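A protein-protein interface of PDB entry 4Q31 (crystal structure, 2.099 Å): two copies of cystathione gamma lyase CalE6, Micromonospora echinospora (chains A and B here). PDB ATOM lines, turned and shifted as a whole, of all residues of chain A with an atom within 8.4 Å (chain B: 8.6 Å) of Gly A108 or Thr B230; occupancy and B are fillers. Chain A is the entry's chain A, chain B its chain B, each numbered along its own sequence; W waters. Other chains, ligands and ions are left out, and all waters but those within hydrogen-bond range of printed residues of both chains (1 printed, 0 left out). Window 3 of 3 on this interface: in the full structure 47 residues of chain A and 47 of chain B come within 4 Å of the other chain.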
ATOM      1  N   SER A  78      18.733 -25.703 -14.176  1.00  0.00           N
ATOM      2  CA  SER A  78      18.560 -24.379 -14.777  1.00  0.00           C
ATOM      3  C   SER A  78      19.684 -23.482 -14.317  1.00  0.00           C
ATOM      4  O   SER A  78      20.367 -23.807 -13.354  1.00  0.00           O
ATOM      5  CB  SER A  78      17.224 -23.744 -14.370  1.00  0.00           C
ATOM      6  OG  SER A  78      17.183 -23.465 -12.977  1.00  0.00           O
ATOM      7  N   GLY A  79      19.883 -22.362 -15.008  1.00  0.00           N
ATOM      8  CA  GLY A  79      20.817 -21.347 -14.543  1.00  0.00           C
ATOM      9  C   GLY A  79      20.458 -20.871 -13.134  1.00  0.00           C
ATOM     10  O   GLY A  79      21.326 -20.767 -12.274  1.00  0.00           O
ATOM     11  N   GLN A  80      19.183 -20.577 -12.897  1.00  0.00           N
ATOM     12  CA  GLN A  80      18.738 -20.179 -11.557  1.00  0.00           C
ATOM     13  C   GLN A  80      19.190 -21.157 -10.460  1.00  0.00           C
ATOM     14  O   GLN A  80      19.579 -20.743  -9.352  1.00  0.00           O
ATOM     15  CB  GLN A  80      17.211 -20.054 -11.510  1.00  0.00           C
ATOM     16  CG  GLN A  80      16.631 -18.799 -12.151  1.00  0.00           C
ATOM     17  CD  GLN A  80      17.139 -17.516 -11.522  1.00  0.00           C
ATOM     18  OE1 GLN A  80      17.889 -16.773 -12.145  1.00  0.00           O
ATOM     19  NE2 GLN A  80      16.716 -17.242 -10.283  1.00  0.00           N
ATOM     20  N   ALA A  81      19.138 -22.448 -10.768  1.00  0.00           N
ATOM     21  CA  ALA A  81      19.500 -23.477  -9.797  1.00  0.00           C
ATOM     22  C   ALA A  81      20.990 -23.475  -9.493  1.00  0.00           C
ATOM     23  O   ALA A  81      21.398 -23.723  -8.362  1.00  0.00           O
ATOM     24  CB  ALA A  81      19.050 -24.857 -10.275  1.00  0.00           C
ATOM     25  N   ALA A  82      21.795 -23.208 -10.511  1.00  0.00           N
ATOM     26  CA  ALA A  82      23.233 -23.045 -10.333  1.00  0.00           C
ATOM     27  C   ALA A  82      23.525 -21.859  -9.411  1.00  0.00           C
ATOM     28  O   ALA A  82      24.343 -21.959  -8.501  1.00  0.00           O
ATOM     29  CB  ALA A  82      23.904 -22.837 -11.682  1.00  0.00           C
ATOM     30  N   ALA A  83      22.844 -20.740  -9.659  1.00  0.00           N
ATOM     31  CA  ALA A  83      23.002 -19.544  -8.837  1.00  0.00           C
ATOM     32  C   ALA A  83      22.515 -19.781  -7.407  1.00  0.00           C
ATOM     33  O   ALA A  83      23.157 -19.341  -6.444  1.00  0.00           O
ATOM     34  CB  ALA A  83      22.259 -18.364  -9.469  1.00  0.00           C
ATOM     35  N   ALA A  84      21.384 -20.470  -7.271  1.00  0.00           N
ATOM     36  CA  ALA A  84      20.814 -20.746  -5.958  1.00  0.00           C
ATOM     37  C   ALA A  84      21.784 -21.586  -5.132  1.00  0.00           C
ATOM     38  O   ALA A  84      21.975 -21.349  -3.939  1.00  0.00           O
ATOM     39  CB  ALA A  84      19.463 -21.459  -6.084  1.00  0.00           C
ATOM     40  N   THR A  85      22.404 -22.555  -5.792  1.00  0.00           N
ATOM     41  CA  THR A  85      23.346 -23.452  -5.144  1.00  0.00           C
ATOM     42  C   THR A  85      24.517 -22.678  -4.572  1.00  0.00           C
ATOM     43  O   THR A  85      24.896 -22.869  -3.414  1.00  0.00           O
ATOM     44  CB  THR A  85      23.822 -24.527  -6.141  1.00  0.00           C
ATOM     45  OG1 THR A  85      22.696 -25.339  -6.493  1.00  0.00           O
ATOM     46  CG2 THR A  85      24.919 -25.403  -5.531  1.00  0.00           C
ATOM     47  N   LEU A  87      24.661 -19.418  -3.907  1.00  0.00           N
ATOM     48  CA  LEU A  87      24.190 -18.528  -2.851  1.00  0.00           C
ATOM     49  C   LEU A  87      23.916 -19.247  -1.529  1.00  0.00           C
ATOM     50  O   LEU A  87      23.980 -18.630  -0.469  1.00  0.00           O
ATOM     51  CB  LEU A  87      22.921 -17.797  -3.282  1.00  0.00           C
ATOM     52  CG  LEU A  87      23.080 -16.405  -3.885  1.00  0.00           C
ATOM     53  CD1 LEU A  87      21.703 -15.838  -4.191  1.00  0.00           C
ATOM     54  CD2 LEU A  87      23.862 -15.483  -2.941  1.00  0.00           C
ATOM     55  N   VAL A 102      22.110  -6.547 -12.020  1.00  0.00           N
ATOM     56  CA  VAL A 102      22.197  -7.991 -12.122  1.00  0.00           C
ATOM     57  C   VAL A 102      20.861  -8.547 -12.650  1.00  0.00           C
ATOM     58  O   VAL A 102      19.816  -7.882 -12.560  1.00  0.00           O
ATOM     59  CB  VAL A 102      22.551  -8.585 -10.744  1.00  0.00           C
ATOM     60  CG1 VAL A 102      21.307  -8.702  -9.866  1.00  0.00           C
ATOM     61  CG2 VAL A 102      23.244  -9.914 -10.890  1.00  0.00           C
ATOM     62  N   TYR A 103      20.901  -9.738 -13.235  1.00  0.00           N
ATOM     63  CA  TYR A 103      19.705 -10.363 -13.810  1.00  0.00           C
ATOM     64  C   TYR A 103      18.592 -10.455 -12.777  1.00  0.00           C
ATOM     65  O   TYR A 103      18.848 -10.785 -11.618  1.00  0.00           O
ATOM     66  CB  TYR A 103      20.045 -11.766 -14.332  1.00  0.00           C
ATOM     67  CG  TYR A 103      18.849 -12.596 -14.762  1.00  0.00           C
ATOM     68  CD1 TYR A 103      17.932 -12.106 -15.685  1.00  0.00           C
ATOM     69  CD2 TYR A 103      18.653 -13.881 -14.262  1.00  0.00           C
ATOM     70  CE1 TYR A 103      16.846 -12.861 -16.085  1.00  0.00           C
ATOM     71  CE2 TYR A 103      17.568 -14.648 -14.660  1.00  0.00           C
ATOM     72  CZ  TYR A 103      16.672 -14.132 -15.579  1.00  0.00           C
ATOM     73  OH  TYR A 103      15.592 -14.885 -15.981  1.00  0.00           O
ATOM     74  N   ALA A 104      17.366 -10.151 -13.194  1.00  0.00           N
ATOM     75  CA  ALA A 104      16.224 -10.178 -12.285  1.00  0.00           C
ATOM     76  C   ALA A 104      16.107 -11.499 -11.511  1.00  0.00           C
ATOM     77  O   ALA A 104      15.705 -11.508 -10.352  1.00  0.00           O
ATOM     78  CB  ALA A 104      14.935  -9.872 -13.033  1.00  0.00           C
ATOM     79  N   GLY A 105      16.463 -12.608 -12.151  1.00  0.00           N
ATOM     80  CA  GLY A 105      16.432 -13.895 -11.478  1.00  0.00           C
ATOM     81  C   GLY A 105      17.454 -13.971 -10.355  1.00  0.00           C
ATOM     82  O   GLY A 105      17.191 -14.527  -9.283  1.00  0.00           O
ATOM     83  N   THR A 106      18.629 -13.410 -10.604  1.00  0.00           N
ATOM     84  CA  THR A 106      19.659 -13.347  -9.585  1.00  0.00           C
ATOM     85  C   THR A 106      19.163 -12.488  -8.416  1.00  0.00           C
ATOM     86  O   THR A 106      19.315 -12.854  -7.259  1.00  0.00           O
ATOM     87  CB  THR A 106      20.964 -12.779 -10.149  1.00  0.00           C
ATOM     88  OG1 THR A 106      21.395 -13.575 -11.263  1.00  0.00           O
ATOM     89  CG2 THR A 106      22.050 -12.781  -9.080  1.00  0.00           C
ATOM     90  N   ASP A 107      18.536 -11.360  -8.729  1.00  0.00           N
ATOM     91  CA  ASP A 107      18.023 -10.471  -7.693  1.00  0.00           C
ATOM     92  C   ASP A 107      16.882 -11.125  -6.896  1.00  0.00           C
ATOM     93  O   ASP A 107      16.729 -10.861  -5.702  1.00  0.00           O
ATOM     94  CB  ASP A 107      17.576  -9.147  -8.300  1.00  0.00           C
ATOM     95  CG  ASP A 107      17.714  -7.992  -7.331  1.00  0.00           C
ATOM     96  OD1 ASP A 107      18.782  -7.871  -6.694  1.00  0.00           O
ATOM     97  OD2 ASP A 107      16.755  -7.211  -7.196  1.00  0.00           O
ATOM     98  N   GLY A 108      16.093 -11.973  -7.554  1.00  0.00           N
ATOM     99  CA  GLY A 108      15.065 -12.751  -6.876  1.00  0.00           C
ATOM    100  C   GLY A 108      15.691 -13.677  -5.842  1.00  0.00           C
ATOM    101  O   GLY A 108      15.195 -13.816  -4.716  1.00  0.00           O
ATOM    102  N   LEU A 109      16.805 -14.293  -6.223  1.00  0.00           N
ATOM    103  CA  LEU A 109      17.564 -15.150  -5.317  1.00  0.00           C
ATOM    104  C   LEU A 109      18.228 -14.347  -4.196  1.00  0.00           C
ATOM    105  O   LEU A 109      18.257 -14.797  -3.052  1.00  0.00           O
ATOM    106  CB  LEU A 109      18.603 -15.988  -6.076  1.00  0.00           C
ATOM    107  CG  LEU A 109      18.065 -17.202  -6.850  1.00  0.00           C
ATOM    108  CD1 LEU A 109      19.121 -17.755  -7.781  1.00  0.00           C
ATOM    109  CD2 LEU A 109      17.586 -18.288  -5.887  1.00  0.00           C
ATOM    110  N   PHE A 110      18.749 -13.165  -4.520  1.00  0.00           N
ATOM    111  CA  PHE A 110      19.290 -12.267  -3.493  1.00  0.00           C
ATOM    112  C   PHE A 110      18.217 -11.924  -2.448  1.00  0.00           C
ATOM    113  O   PHE A 110      18.494 -11.890  -1.250  1.00  0.00           O
ATOM    114  CB  PHE A 110      19.825 -10.976  -4.119  1.00  0.00           C
ATOM    115  CG  PHE A 110      21.112 -11.146  -4.894  1.00  0.00           C
ATOM    116  CD1 PHE A 110      21.870 -12.306  -4.780  1.00  0.00           C
ATOM    117  CD2 PHE A 110      21.568 -10.133  -5.729  1.00  0.00           C
ATOM    118  CE1 PHE A 110      23.059 -12.454  -5.482  1.00  0.00           C
ATOM    119  CE2 PHE A 110      22.757 -10.270  -6.437  1.00  0.00           C
ATOM    120  CZ  PHE A 110      23.507 -11.436  -6.310  1.00  0.00           C
ATOM    121  N   ASP A 111      16.992 -11.682  -2.914  1.00  0.00           N
ATOM    122  CA  ASP A 111      15.871 -11.363  -2.032  1.00  0.00           C
ATOM    123  C   ASP A 111      15.528 -12.538  -1.132  1.00  0.00           C
ATOM    124  O   ASP A 111      15.237 -12.359   0.050  1.00  0.00           O
ATOM    125  CB  ASP A 111      14.628 -10.976  -2.836  1.00  0.00           C
ATOM    126  CG  ASP A 111      14.775  -9.640  -3.535  1.00  0.00           C
ATOM    127  OD1 ASP A 111      15.612  -8.819  -3.097  1.00  0.00           O
ATOM    128  OD2 ASP A 111      14.048  -9.415  -4.529  1.00  0.00           O
ATOM    129  N   LEU A 112      15.562 -13.739  -1.700  1.00  0.00           N
ATOM    130  CA  LEU A 112      15.278 -14.950  -0.944  1.00  0.00           C
ATOM    131  C   LEU A 112      16.322 -15.110   0.165  1.00  0.00           C
ATOM    132  O   LEU A 112      15.988 -15.369   1.331  1.00  0.00           O
ATOM    133  CB  LEU A 112      15.277 -16.161  -1.887  1.00  0.00           C
ATOM    134  CG  LEU A 112      14.348 -17.335  -1.595  1.00  0.00           C
ATOM    135  CD1 LEU A 112      12.902 -16.881  -1.405  1.00  0.00           C
ATOM    136  CD2 LEU A 112      14.449 -18.365  -2.711  1.00  0.00           C
ATOM    137  N   ALA A 113      17.584 -14.921  -0.203  1.00  0.00           N
ATOM    138  CA  ALA A 113      18.690 -15.004   0.737  1.00  0.00           C
ATOM    139  C   ALA A 113      18.589 -13.920   1.810  1.00  0.00           C
ATOM    140  O   ALA A 113      18.857 -14.172   2.987  1.00  0.00           O
ATOM    141  CB  ALA A 113      20.016 -14.893  -0.006  1.00  0.00           C
ATOM    142  N   ALA A 114      18.197 -12.719   1.404  1.00  0.00           N
ATOM    143  CA  ALA A 114      18.073 -11.611   2.350  1.00  0.00           C
ATOM    144  C   ALA A 114      17.000 -11.892   3.393  1.00  0.00           C
ATOM    145  O   ALA A 114      17.061 -11.363   4.498  1.00  0.00           O
ATOM    146  CB  ALA A 114      17.782 -10.301   1.627  1.00  0.00           C
ATOM    147  N   ARG A 115      16.024 -12.735   3.049  1.00  0.00           N
ATOM    148  CA  ARG A 115      14.959 -13.068   3.994  1.00  0.00           C
ATOM    149  C   ARG A 115      15.407 -14.153   4.960  1.00  0.00           C
ATOM    150  O   ARG A 115      14.710 -14.471   5.924  1.00  0.00           O
ATOM    151  CB  ARG A 115      13.671 -13.468   3.272  1.00  0.00           C
ATOM    152  CG  ARG A 115      13.052 -12.330   2.486  1.00  0.00           C
ATOM    153  CD  ARG A 115      11.645 -12.650   2.022  1.00  0.00           C
ATOM    154  NE  ARG A 115      11.405 -12.165   0.664  1.00  0.00           N
ATOM    155  CZ  ARG A 115      11.172 -10.895   0.343  1.00  0.00           C
ATOM    156  NH1 ARG A 115      10.969 -10.560  -0.926  1.00  0.00           N
ATOM    157  NH2 ARG A 115      11.146  -9.957   1.282  1.00  0.00           N
ATOM    158  N   TYR A 122      24.442  -3.680  -2.922  1.00  0.00           N
ATOM    159  CA  TYR A 122      24.641  -3.349  -4.325  1.00  0.00           C
ATOM    160  C   TYR A 122      25.660  -2.234  -4.436  1.00  0.00           C
ATOM    161  O   TYR A 122      25.687  -1.316  -3.613  1.00  0.00           O
ATOM    162  CB  TYR A 122      23.326  -2.950  -4.995  1.00  0.00           C
ATOM    163  CG  TYR A 122      22.273  -4.031  -4.934  1.00  0.00           C
ATOM    164  CD1 TYR A 122      22.178  -4.992  -5.928  1.00  0.00           C
ATOM    165  CD2 TYR A 122      21.382  -4.094  -3.871  1.00  0.00           C
ATOM    166  CE1 TYR A 122      21.215  -5.989  -5.869  1.00  0.00           C
ATOM    167  CE2 TYR A 122      20.420  -5.085  -3.800  1.00  0.00           C
ATOM    168  CZ  TYR A 122      20.338  -6.027  -4.800  1.00  0.00           C
ATOM    169  OH  TYR A 122      19.380  -7.013  -4.722  1.00  0.00           O
ATOM    170  N1  LLP A 200      21.819 -15.378 -15.633  1.00  0.00           N
ATOM    171  C2  LLP A 200      21.764 -14.828 -16.978  1.00  0.00           C
ATOM    172  C2' LLP A 200      22.783 -13.772 -17.402  1.00  0.00           C
ATOM    173  C3  LLP A 200      20.806 -15.285 -17.840  1.00  0.00           C
ATOM    174  O3  LLP A 200      20.759 -14.764 -19.134  1.00  0.00           O
ATOM    175  C4  LLP A 200      19.823 -16.326 -17.408  1.00  0.00           C
ATOM    176  C4' LLP A 200      18.739 -16.848 -18.392  1.00  0.00           C
ATOM    177  C5  LLP A 200      19.893 -16.798 -16.162  1.00  0.00           C
ATOM    178  C6  LLP A 200      20.951 -16.304 -15.225  1.00  0.00           C
ATOM    179  C5' LLP A 200      18.925 -17.830 -15.612  1.00  0.00           C
ATOM    180  OP4 LLP A 200      19.196 -19.100 -16.139  1.00  0.00           O
ATOM    181  P   LLP A 200      17.938 -20.026 -16.383  1.00  0.00           P
ATOM    182  OP1 LLP A 200      18.391 -21.211 -17.122  1.00  0.00           O
ATOM    183  OP2 LLP A 200      17.293 -20.521 -15.142  1.00  0.00           O
ATOM    184  OP3 LLP A 200      16.842 -19.364 -17.128  1.00  0.00           O
ATOM    185  N   LLP A 200      20.986 -20.762 -22.579  1.00  0.00           N
ATOM    186  CA  LLP A 200      21.232 -19.741 -23.570  1.00  0.00           C
ATOM    187  CB  LLP A 200      21.692 -18.459 -22.878  1.00  0.00           C
ATOM    188  CG  LLP A 200      20.823 -18.223 -21.634  1.00  0.00           C
ATOM    189  CD  LLP A 200      19.463 -17.574 -21.958  1.00  0.00           C
ATOM    190  CE  LLP A 200      18.561 -17.516 -20.702  1.00  0.00           C
ATOM    191  NZ  LLP A 200      19.002 -16.475 -19.774  1.00  0.00           N
ATOM    192  C   LLP A 200      22.174 -20.219 -24.670  1.00  0.00           C
ATOM    193  O   LLP A 200      21.818 -21.193 -25.375  1.00  0.00           O
ATOM    194  N   ARG B  51      11.239 -21.835 -18.011  1.00  0.00           N
ATOM    195  CA  ARG B  51      11.358 -22.082 -16.572  1.00  0.00           C
ATOM    196  C   ARG B  51      10.021 -21.790 -15.890  1.00  0.00           C
ATOM    197  O   ARG B  51       9.633 -22.474 -14.940  1.00  0.00           O
ATOM    198  CB  ARG B  51      12.494 -21.260 -15.933  1.00  0.00           C
ATOM    199  CG  ARG B  51      12.551 -21.366 -14.389  1.00  0.00           C
ATOM    200  CD  ARG B  51      13.917 -20.990 -13.800  1.00  0.00           C
ATOM    201  NE  ARG B  51      14.634 -19.996 -14.600  1.00  0.00           N
ATOM    202  CZ  ARG B  51      14.381 -18.692 -14.592  1.00  0.00           C
ATOM    203  NH1 ARG B  51      15.087 -17.875 -15.368  1.00  0.00           N
ATOM    204  NH2 ARG B  51      13.407 -18.207 -13.824  1.00  0.00           N
ATOM    205  N   GLY B  52       9.314 -20.782 -16.393  1.00  0.00           N
ATOM    206  CA  GLY B  52       8.044 -20.375 -15.806  1.00  0.00           C
ATOM    207  C   GLY B  52       6.862 -21.178 -16.347  1.00  0.00           C
ATOM    208  O   GLY B  52       6.015 -21.645 -15.593  1.00  0.00           O
ATOM    209  N   ALA B 223       2.932 -19.370  -3.577  1.00  0.00           N
ATOM    210  CA  ALA B 223       4.257 -19.443  -2.954  1.00  0.00           C
ATOM    211  C   ALA B 223       5.114 -20.564  -3.559  1.00  0.00           C
ATOM    212  O   ALA B 223       6.307 -20.383  -3.814  1.00  0.00           O
ATOM    213  CB  ALA B 223       4.142 -19.609  -1.452  1.00  0.00           C
ATOM    214  N   VAL B 224       4.505 -21.718  -3.784  1.00  0.00           N
ATOM    215  CA  VAL B 224       5.211 -22.841  -4.398  1.00  0.00           C
ATOM    216  C   VAL B 224       5.685 -22.516  -5.832  1.00  0.00           C
ATOM    217  O   VAL B 224       6.831 -22.807  -6.197  1.00  0.00           O
ATOM    218  CB  VAL B 224       4.345 -24.110  -4.403  1.00  0.00           C
ATOM    219  CG1 VAL B 224       4.872 -25.122  -5.396  1.00  0.00           C
ATOM    220  CG2 VAL B 224       4.264 -24.711  -2.984  1.00  0.00           C
ATOM    221  N   ARG B 225       4.823 -21.902  -6.638  1.00  0.00           N
ATOM    222  CA  ARG B 225       5.211 -21.597  -8.017  1.00  0.00           C
ATOM    223  C   ARG B 225       6.283 -20.513  -8.042  1.00  0.00           C
ATOM    224  O   ARG B 225       7.212 -20.569  -8.841  1.00  0.00           O
ATOM    225  CB  ARG B 225       4.000 -21.205  -8.885  1.00  0.00           C
ATOM    226  CG  ARG B 225       3.079 -22.380  -9.237  1.00  0.00           C
ATOM    227  CD  ARG B 225       3.819 -23.467 -10.006  1.00  0.00           C
ATOM    228  NE  ARG B 225       2.958 -24.616 -10.300  1.00  0.00           N
ATOM    229  CZ  ARG B 225       2.125 -24.682 -11.334  1.00  0.00           C
ATOM    230  NH1 ARG B 225       2.043 -23.663 -12.177  1.00  0.00           N
ATOM    231  NH2 ARG B 225       1.364 -25.762 -11.522  1.00  0.00           N
ATOM    232  N   ALA B 226       6.168 -19.536  -7.150  1.00  0.00           N
ATOM    233  CA  ALA B 226       7.174 -18.487  -7.077  1.00  0.00           C
ATOM    234  C   ALA B 226       8.541 -19.058  -6.703  1.00  0.00           C
ATOM    235  O   ALA B 226       9.567 -18.625  -7.224  1.00  0.00           O
ATOM    236  CB  ALA B 226       6.764 -17.408  -6.083  1.00  0.00           C
ATOM    237  N   TYR B 227       8.552 -20.016  -5.785  1.00  0.00           N
ATOM    238  CA  TYR B 227       9.807 -20.621  -5.366  1.00  0.00           C
ATOM    239  C   TYR B 227      10.441 -21.462  -6.470  1.00  0.00           C
ATOM    240  O   TYR B 227      11.654 -21.401  -6.695  1.00  0.00           O
ATOM    241  CB  TYR B 227       9.621 -21.463  -4.103  1.00  0.00           C
ATOM    242  CG  TYR B 227      10.924 -22.030  -3.599  1.00  0.00           C
ATOM    243  CD1 TYR B 227      11.735 -21.299  -2.730  1.00  0.00           C
ATOM    244  CD2 TYR B 227      11.355 -23.291  -3.996  1.00  0.00           C
ATOM    245  CE1 TYR B 227      12.936 -21.816  -2.271  1.00  0.00           C
ATOM    246  CE2 TYR B 227      12.548 -23.815  -3.543  1.00  0.00           C
ATOM    247  CZ  TYR B 227      13.334 -23.069  -2.680  1.00  0.00           C
ATOM    248  OH  TYR B 227      14.516 -23.596  -2.223  1.00  0.00           O
ATOM    249  N   ARG B 228       9.622 -22.259  -7.152  1.00  0.00           N
ATOM    250  CA  ARG B 228      10.133 -23.100  -8.222  1.00  0.00           C
ATOM    251  C   ARG B 228      10.773 -22.235  -9.299  1.00  0.00           C
ATOM    252  O   ARG B 228      11.854 -22.538  -9.798  1.00  0.00           O
ATOM    253  CB  ARG B 228       9.024 -23.963  -8.836  1.00  0.00           C
ATOM    254  CG  ARG B 228       9.594 -25.029  -9.790  1.00  0.00           C
ATOM    255  CD  ARG B 228       8.515 -25.846 -10.495  1.00  0.00           C
ATOM    256  NE  ARG B 228       7.674 -24.993 -11.314  1.00  0.00           N
ATOM    257  CZ  ARG B 228       6.652 -25.429 -12.037  1.00  0.00           C
ATOM    258  NH1 ARG B 228       6.351 -26.729 -12.057  1.00  0.00           N
ATOM    259  NH2 ARG B 228       5.943 -24.567 -12.755  1.00  0.00           N
ATOM    260  N   THR B 229      10.099 -21.142  -9.640  1.00  0.00           N
ATOM    261  CA  THR B 229      10.574 -20.231 -10.671  1.00  0.00           C
ATOM    262  C   THR B 229      11.899 -19.573 -10.288  1.00  0.00           C
ATOM    263  O   THR B 229      12.801 -19.435 -11.113  1.00  0.00           O
ATOM    264  CB  THR B 229       9.520 -19.141 -10.968  1.00  0.00           C
ATOM    265  OG1 THR B 229       8.332 -19.759 -11.489  1.00  0.00           O
ATOM    266  CG2 THR B 229      10.053 -18.144 -11.987  1.00  0.00           C
ATOM    267  N   THR B 230      12.018 -19.178  -9.029  1.00  0.00           N
ATOM    268  CA  THR B 230      13.226 -18.517  -8.550  1.00  0.00           C
ATOM    269  C   THR B 230      14.400 -19.482  -8.287  1.00  0.00           C
ATOM    270  O   THR B 230      15.530 -19.209  -8.686  1.00  0.00           O
ATOM    271  CB  THR B 230      12.916 -17.698  -7.289  1.00  0.00           C
ATOM    272  OG1 THR B 230      11.926 -16.713  -7.614  1.00  0.00           O
ATOM    273  CG2 THR B 230      14.169 -17.009  -6.762  1.00  0.00           C
ATOM    274  N   ALA B 231      14.128 -20.604  -7.623  1.00  0.00           N
ATOM    275  CA  ALA B 231      15.153 -21.617  -7.359  1.00  0.00           C
ATOM    276  C   ALA B 231      15.499 -22.425  -8.616  1.00  0.00           C
ATOM    277  O   ALA B 231      16.598 -22.962  -8.733  1.00  0.00           O
ATOM    278  CB  ALA B 231      14.707 -22.545  -6.236  1.00  0.00           C
ATOM    279  N   GLY B 232      14.555 -22.512  -9.547  1.00  0.00           N
ATOM    280  CA  GLY B 232      14.813 -23.116 -10.850  1.00  0.00           C
ATOM    281  C   GLY B 232      14.914 -24.628 -10.827  1.00  0.00           C
ATOM    282  O   GLY B 232      15.542 -25.230 -11.707  1.00  0.00           O
ATOM    283  N   ASN B 233      14.304 -25.244  -9.815  1.00  0.00           N
ATOM    284  CA  ASN B 233      14.300 -26.696  -9.692  1.00  0.00           C
ATOM    285  C   ASN B 233      13.188 -27.319 -10.535  1.00  0.00           C
ATOM    286  O   ASN B 233      12.405 -28.146 -10.054  1.00  0.00           O
ATOM    287  CB  ASN B 233      14.202 -27.130  -8.217  1.00  0.00           C
ATOM    288  CG  ASN B 233      13.080 -26.418  -7.453  1.00  0.00           C
ATOM    289  OD1 ASN B 233      12.293 -25.652  -8.022  1.00  0.00           O
ATOM    290  ND2 ASN B 233      13.007 -26.679  -6.151  1.00  0.00           N
ATOM    291  N   VAL B 234      13.132 -26.914 -11.800  1.00  0.00           N
ATOM    292  CA  VAL B 234      12.081 -27.347 -12.723  1.00  0.00           C
ATOM    293  C   VAL B 234      12.536 -28.549 -13.530  1.00  0.00           C
ATOM    294  O   VAL B 234      13.703 -28.630 -13.883  1.00  0.00           O
ATOM    295  CB  VAL B 234      11.755 -26.230 -13.719  1.00  0.00           C
ATOM    296  CG1 VAL B 234      11.031 -25.121 -13.035  1.00  0.00           C
ATOM    297  CG2 VAL B 234      13.037 -25.689 -14.333  1.00  0.00           C
HETATM  298  O   HOH W   1      13.026 -15.393 -13.819  1.00  0.00           O
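No position is printed for both chains.
OG of Ser A78 lies within hydrogen-bond range of N of Ala A81 (3.1 Å).
N of Gly A79 is in hydrogen-bond range of OP1 of LLP A200, 2.8 Å away.
NE2 of Gln A80 sits at hydrogen-bond distance from O of Gly A105, at 2.9 Å.
The backbone NH of Gln A80 is in hydrogen-bond range of OP2 of LLP A200, 2.9 Å away.
OG1 of Thr A85 is in hydrogen-bond range of O of Ala A81 (2.8 Å).
The backbone carbonyl oxygen of Ala B226 lies within hydrogen-bond range of the side-chain hydroxyl of Thr B230, 3.1 Å away.
Water W1 lies within hydrogen-bond range of the guanidinium group of Arg B51 (2.8 Å) and the side-chain hydroxyl of Tyr A103 (3.4 Å).
The side-chain hydroxyl (OG) of Ser A78 is in hydrogen-bond range of the backbone carbonyl oxygen (O) of Gly B232 (2.7 Å).
NE2 of Gln A80 is in hydrogen-bond range of O of Thr B230.
The backbone carbonyl oxygen (O) of Ala B231 lies close to the backbone NH (N) of Ala A81.
The side-chain hydroxyl of Tyr A103 lies within hydrogen-bond range of the guanidinium group of Arg B51, at 3.1 Å.
NE of Arg B51 sits close to OP2 of LLP A200 (2.8 Å).
CG of Gln A80 touches CZ of Arg B51, 3.3 Å away.
C of Gln A80 touches O of Ala B231, 3.6 Å away.
CA of Gly B232 touches CB of Gln A80 (3.9 Å).
CB of Ala A81 touches O of Gly B232 (3.8 Å).
CG2 of Thr B230 touches C of Gly A108, 3.8 Å away.
CD2 of Leu A109 touches O of Thr B230, 3.6 Å away.
Leu A112 touches Tyr B227.
Of the printed residues of chain B, Leu A109 touches Thr B230.
Of chain A, only Gln A80 and Ala A81 come within 4 Å of Ala B231.
Printed residues of chain B within 4 Å of Ala A81: Ala B231 and Gly B232.
Printed residues of chain B within 4 Å of Gln A80: Arg B51 (3.3 Å), Thr B230 (2.8 Å), Ala B231 (3.6 Å) and Gly B232 (3.9 Å).
Of the printed residues of chain B, Tyr A103 touches Arg B51.
Of the printed residues of chain B, Leu A112 touches Tyr B227.
Of the printed residues of chain A, Tyr B227 touches Leu A112 (3.8 Å).
The nearest residue of chain A that does not touch Thr B230 is Leu A112 (4.3 Å).
Of the 14 printed residues of chain B, 5 touch a printed residue of chain A.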
